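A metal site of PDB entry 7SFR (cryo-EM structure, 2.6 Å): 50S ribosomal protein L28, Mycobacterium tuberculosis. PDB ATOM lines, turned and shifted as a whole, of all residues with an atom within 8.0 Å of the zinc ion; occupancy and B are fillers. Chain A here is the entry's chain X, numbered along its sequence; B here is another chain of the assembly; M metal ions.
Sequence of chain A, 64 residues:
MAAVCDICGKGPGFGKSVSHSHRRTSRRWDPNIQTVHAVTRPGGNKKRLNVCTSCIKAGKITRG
Of the 20 residues printed, 4 come within 4 Å of the zinc ion.
The zinc ion is bound by the side-chain sulfur of Cys 8 (2.3 Å), the side-chain sulfur of Cys 52 (2.3 Å), the side-chain sulfur of Cys 5 (2.3 Å) and the side-chain sulfur of Cys 55 (2.3 Å). The zinc ion has four donor atoms within binding distance.
SG of Cys 8 lies close to N of Lys 10 (3.6 Å). SG of Cys 5 lies close to N of Ile 7 (3.3 Å). N of Cys 5 is in hydrogen-bond range of O of Lys 10, at 3.1 Å.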
ATOM      1  N   VAL A   4     -27.712   1.741  11.953  1.00  0.00           N
ATOM      2  CA  VAL A   4     -27.618   0.284  11.922  1.00  0.00           C
ATOM      3  C   VAL A   4     -26.150  -0.115  11.918  1.00  0.00           C
ATOM      4  O   VAL A   4     -25.351   0.460  11.171  1.00  0.00           O
ATOM      5  CB  VAL A   4     -28.353  -0.310  10.700  1.00  0.00           C
ATOM      6  CG1 VAL A   4     -28.459  -1.810  10.834  1.00  0.00           C
ATOM      7  CG2 VAL A   4     -29.723   0.300  10.540  1.00  0.00           C
ATOM      8  N   CYS A   5     -25.805  -1.096  12.746  1.00  0.00           N
ATOM      9  CA  CYS A   5     -24.432  -1.581  12.830  1.00  0.00           C
ATOM     10  C   CYS A   5     -24.161  -2.553  11.698  1.00  0.00           C
ATOM     11  O   CYS A   5     -24.994  -3.414  11.390  1.00  0.00           O
ATOM     12  CB  CYS A   5     -24.159  -2.259  14.172  1.00  0.00           C
ATOM     13  SG  CYS A   5     -22.507  -2.981  14.310  1.00  0.00           S
ATOM     14  N   ASP A   6     -22.990  -2.423  11.072  1.00  0.00           N
ATOM     15  CA  ASP A   6     -22.639  -3.281   9.948  1.00  0.00           C
ATOM     16  C   ASP A   6     -22.199  -4.669  10.382  1.00  0.00           C
ATOM     17  O   ASP A   6     -22.256  -5.604   9.575  1.00  0.00           O
ATOM     18  CB  ASP A   6     -21.543  -2.637   9.118  1.00  0.00           C
ATOM     19  CG  ASP A   6     -22.066  -1.551   8.211  1.00  0.00           C
ATOM     20  OD1 ASP A   6     -23.295  -1.498   8.003  1.00  0.00           O
ATOM     21  OD2 ASP A   6     -21.255  -0.737   7.710  1.00  0.00           O
ATOM     22  N   ILE A   7     -21.767  -4.840  11.634  1.00  0.00           N
ATOM     23  CA  ILE A   7     -21.239  -6.121  12.066  1.00  0.00           C
ATOM     24  C   ILE A   7     -22.335  -6.946  12.727  1.00  0.00           C
ATOM     25  O   ILE A   7     -22.693  -8.026  12.243  1.00  0.00           O
ATOM     26  CB  ILE A   7     -20.052  -5.933  13.031  1.00  0.00           C
ATOM     27  CG1 ILE A   7     -18.991  -5.040  12.381  1.00  0.00           C
ATOM     28  CG2 ILE A   7     -19.464  -7.271  13.406  1.00  0.00           C
ATOM     29  CD1 ILE A   7     -18.114  -5.758  11.410  1.00  0.00           C
ATOM     30  N   CYS A   8     -22.868  -6.451  13.839  1.00  0.00           N
ATOM     31  CA  CYS A   8     -23.845  -7.200  14.614  1.00  0.00           C
ATOM     32  C   CYS A   8     -25.292  -6.924  14.204  1.00  0.00           C
ATOM     33  O   CYS A   8     -26.199  -7.587  14.691  1.00  0.00           O
ATOM     34  CB  CYS A   8     -23.675  -6.908  16.114  1.00  0.00           C
ATOM     35  SG  CYS A   8     -24.135  -5.254  16.640  1.00  0.00           S
ATOM     36  N   GLY A   9     -25.517  -5.964  13.313  1.00  0.00           N
ATOM     37  CA  GLY A   9     -26.861  -5.694  12.835  1.00  0.00           C
ATOM     38  C   GLY A   9     -27.764  -4.999  13.815  1.00  0.00           C
ATOM     39  O   GLY A   9     -28.974  -4.918  13.575  1.00  0.00           O
ATOM     40  N   LYS A  10     -27.233  -4.493  14.922  1.00  0.00           N
ATOM     41  CA  LYS A  10     -28.052  -3.831  15.930  1.00  0.00           C
ATOM     42  C   LYS A  10     -28.710  -2.589  15.360  1.00  0.00           C
ATOM     43  O   LYS A  10     -28.048  -1.766  14.716  1.00  0.00           O
ATOM     44  CB  LYS A  10     -27.203  -3.486  17.148  1.00  0.00           C
ATOM     45  CG  LYS A  10     -27.636  -2.247  17.879  1.00  0.00           C
ATOM     46  CD  LYS A  10     -27.293  -2.340  19.342  1.00  0.00           C
ATOM     47  CE  LYS A  10     -25.813  -2.204  19.586  1.00  0.00           C
ATOM     48  NZ  LYS A  10     -25.477  -2.587  20.971  1.00  0.00           N
ATOM     49  N   GLY A  11     -30.010  -2.449  15.582  1.00  0.00           N
ATOM     50  CA  GLY A  11     -30.765  -1.346  15.044  1.00  0.00           C
ATOM     51  C   GLY A  11     -31.386  -0.497  16.134  1.00  0.00           C
ATOM     52  O   GLY A  11     -31.247  -0.779  17.326  1.00  0.00           O
ATOM     53  N   PRO A  31     -28.423   3.375  18.374  1.00  0.00           N
ATOM     54  CA  PRO A  31     -27.122   2.887  18.824  1.00  0.00           C
ATOM     55  C   PRO A  31     -26.021   3.893  18.514  1.00  0.00           C
ATOM     56  O   PRO A  31     -26.135   4.721  17.609  1.00  0.00           O
ATOM     57  CB  PRO A  31     -26.929   1.592  18.042  1.00  0.00           C
ATOM     58  CG  PRO A  31     -27.810   1.706  16.890  1.00  0.00           C
ATOM     59  CD  PRO A  31     -28.957   2.567  17.277  1.00  0.00           C
ATOM     60  N   ASN A  32     -24.956   3.819  19.302  1.00  0.00           N
ATOM     61  CA  ASN A  32     -23.805   4.707  19.125  1.00  0.00           C
ATOM     62  C   ASN A  32     -22.969   4.185  17.972  1.00  0.00           C
ATOM     63  O   ASN A  32     -21.984   3.475  18.158  1.00  0.00           O
ATOM     64  CB  ASN A  32     -22.992   4.787  20.404  1.00  0.00           C
ATOM     65  CG  ASN A  32     -22.124   6.010  20.436  1.00  0.00           C
ATOM     66  OD1 ASN A  32     -22.113   6.797  19.505  1.00  0.00           O
ATOM     67  ND2 ASN A  32     -21.368   6.176  21.520  1.00  0.00           N
ATOM     68  N   ILE A  33     -23.365   4.543  16.748  1.00  0.00           N
ATOM     69  CA  ILE A  33     -22.696   4.087  15.540  1.00  0.00           C
ATOM     70  C   ILE A  33     -21.615   5.091  15.179  1.00  0.00           C
ATOM     71  O   ILE A  33     -21.871   6.300  15.104  1.00  0.00           O
ATOM     72  CB  ILE A  33     -23.690   3.914  14.389  1.00  0.00           C
ATOM     73  CG1 ILE A  33     -24.724   2.849  14.736  1.00  0.00           C
ATOM     74  CG2 ILE A  33     -22.953   3.561  13.120  1.00  0.00           C
ATOM     75  CD1 ILE A  33     -24.148   1.480  14.836  1.00  0.00           C
ATOM     76  N   ASN A  50     -19.897   1.189   9.154  1.00  0.00           N
ATOM     77  CA  ASN A  50     -20.685   1.818  10.214  1.00  0.00           C
ATOM     78  C   ASN A  50     -20.886   0.778  11.307  1.00  0.00           C
ATOM     79  O   ASN A  50     -21.704  -0.127  11.162  1.00  0.00           O
ATOM     80  CB  ASN A  50     -22.025   2.304   9.671  1.00  0.00           C
ATOM     81  CG  ASN A  50     -21.917   3.631   8.972  1.00  0.00           C
ATOM     82  OD1 ASN A  50     -21.047   4.431   9.288  1.00  0.00           O
ATOM     83  ND2 ASN A  50     -22.784   3.862   8.001  1.00  0.00           N
ATOM     84  N   VAL A  51     -20.123   0.887  12.389  1.00  0.00           N
ATOM     85  CA  VAL A  51     -20.190  -0.069  13.477  1.00  0.00           C
ATOM     86  C   VAL A  51     -20.486   0.654  14.782  1.00  0.00           C
ATOM     87  O   VAL A  51     -20.321   1.876  14.889  1.00  0.00           O
ATOM     88  CB  VAL A  51     -18.907  -0.909  13.605  1.00  0.00           C
ATOM     89  CG1 VAL A  51     -18.356  -1.234  12.253  1.00  0.00           C
ATOM     90  CG2 VAL A  51     -17.885  -0.156  14.384  1.00  0.00           C
ATOM     91  N   CYS A  52     -20.934  -0.102  15.760  1.00  0.00           N
ATOM     92  CA  CYS A  52     -21.314   0.450  17.045  1.00  0.00           C
ATOM     93  C   CYS A  52     -20.164   0.361  18.034  1.00  0.00           C
ATOM     94  O   CYS A  52     -19.253  -0.470  17.895  1.00  0.00           O
ATOM     95  CB  CYS A  52     -22.552  -0.251  17.618  1.00  0.00           C
ATOM     96  SG  CYS A  52     -22.357  -2.014  17.963  1.00  0.00           S
ATOM     97  N   THR A  53     -20.209   1.238  19.036  1.00  0.00           N
ATOM     98  CA  THR A  53     -19.118   1.330  19.998  1.00  0.00           C
ATOM     99  C   THR A  53     -18.911   0.033  20.763  1.00  0.00           C
ATOM    100  O   THR A  53     -17.790  -0.227  21.198  1.00  0.00           O
ATOM    101  CB  THR A  53     -19.375   2.468  20.965  1.00  0.00           C
ATOM    102  OG1 THR A  53     -20.764   2.510  21.279  1.00  0.00           O
ATOM    103  CG2 THR A  53     -18.964   3.780  20.348  1.00  0.00           C
ATOM    104  N   SER A  54     -19.950  -0.779  20.928  1.00  0.00           N
ATOM    105  CA  SER A  54     -19.750  -2.075  21.567  1.00  0.00           C
ATOM    106  C   SER A  54     -18.870  -2.975  20.701  1.00  0.00           C
ATOM    107  O   SER A  54     -17.978  -3.654  21.210  1.00  0.00           O
ATOM    108  CB  SER A  54     -21.085  -2.741  21.837  1.00  0.00           C
ATOM    109  OG  SER A  54     -22.041  -1.771  22.237  1.00  0.00           O
ATOM    110  N   CYS A  55     -19.117  -2.981  19.393  1.00  0.00           N
ATOM    111  CA  CYS A  55     -18.276  -3.751  18.495  1.00  0.00           C
ATOM    112  C   CYS A  55     -16.859  -3.194  18.438  1.00  0.00           C
ATOM    113  O   CYS A  55     -15.900  -3.959  18.273  1.00  0.00           O
ATOM    114  CB  CYS A  55     -18.893  -3.804  17.099  1.00  0.00           C
ATOM    115  SG  CYS A  55     -20.323  -4.893  16.949  1.00  0.00           S
ATOM    116  N   ILE A  56     -16.710  -1.871  18.543  1.00  0.00           N
ATOM    117  CA  ILE A  56     -15.375  -1.297  18.623  1.00  0.00           C
ATOM    118  C   ILE A  56     -14.679  -1.732  19.907  1.00  0.00           C
ATOM    119  O   ILE A  56     -13.488  -2.085  19.893  1.00  0.00           O
ATOM    120  CB  ILE A  56     -15.427   0.232  18.520  1.00  0.00           C
ATOM    121  CG1 ILE A  56     -15.958   0.661  17.153  1.00  0.00           C
ATOM    122  CG2 ILE A  56     -14.061   0.820  18.720  1.00  0.00           C
ATOM    123  CD1 ILE A  56     -16.155   2.144  17.032  1.00  0.00           C
ATOM    124  N   LYS A  60     -13.827  -6.732  17.549  1.00  0.00           N
ATOM    125  CA  LYS A  60     -14.508  -7.189  16.350  1.00  0.00           C
ATOM    126  C   LYS A  60     -13.989  -6.546  15.078  1.00  0.00           C
ATOM    127  O   LYS A  60     -14.166  -7.123  13.995  1.00  0.00           O
ATOM    128  CB  LYS A  60     -16.016  -6.940  16.483  1.00  0.00           C
ATOM    129  CG  LYS A  60     -16.776  -8.125  17.025  1.00  0.00           C
ATOM    130  CD  LYS A  60     -18.280  -7.877  17.010  1.00  0.00           C
ATOM    131  CE  LYS A  60     -19.040  -9.115  17.464  1.00  0.00           C
ATOM    132  NZ  LYS A  60     -18.309  -9.845  18.531  1.00  0.00           N
ATOM    133  P     U B 486     -26.224   1.008  22.092  1.00  0.00           P
ATOM    134  OP1   U B 486     -25.320   1.257  20.943  1.00  0.00           O
ATOM    135  OP2   U B 486     -26.239  -0.324  22.724  1.00  0.00           O
ATOM    136  O5'   U B 486     -25.893   2.081  23.205  1.00  0.00           O
ATOM    137  C5'   U B 486     -25.854   3.464  22.914  1.00  0.00           C
ATOM    138  C4'   U B 486     -25.640   4.285  24.154  1.00  0.00           C
ATOM    139  O4'   U B 486     -26.779   4.142  25.037  1.00  0.00           O
ATOM    140  C3'   U B 486     -24.462   3.884  25.026  1.00  0.00           C
ATOM    141  O3'   U B 486     -23.216   4.334  24.550  1.00  0.00           O
ATOM    142  C2'   U B 486     -24.852   4.482  26.370  1.00  0.00           C
ATOM    143  O2'   U B 486     -24.672   5.877  26.363  1.00  0.00           O
ATOM    144  C1'   U B 486     -26.354   4.202  26.378  1.00  0.00           C
ATOM    145  N1    U B 486     -26.657   2.913  27.045  1.00  0.00           N
ATOM    146  C2    U B 486     -26.710   2.919  28.414  1.00  0.00           C
ATOM    147  O2    U B 486     -26.530   3.922  29.073  1.00  0.00           O
ATOM    148  N3    U B 486     -27.001   1.717  28.997  1.00  0.00           N
ATOM    149  C4    U B 486     -27.226   0.531  28.340  1.00  0.00           C
ATOM    150  O4    U B 486     -27.472  -0.483  28.993  1.00  0.00           O
ATOM    151  C5    U B 486     -27.151   0.609  26.920  1.00  0.00           C
ATOM    152  C6    U B 486     -26.883   1.765  26.344  1.00  0.00           C
HETATM  153 ZN    ZN M   1     -22.330  -3.804  16.482  1.00  0.00          ZN
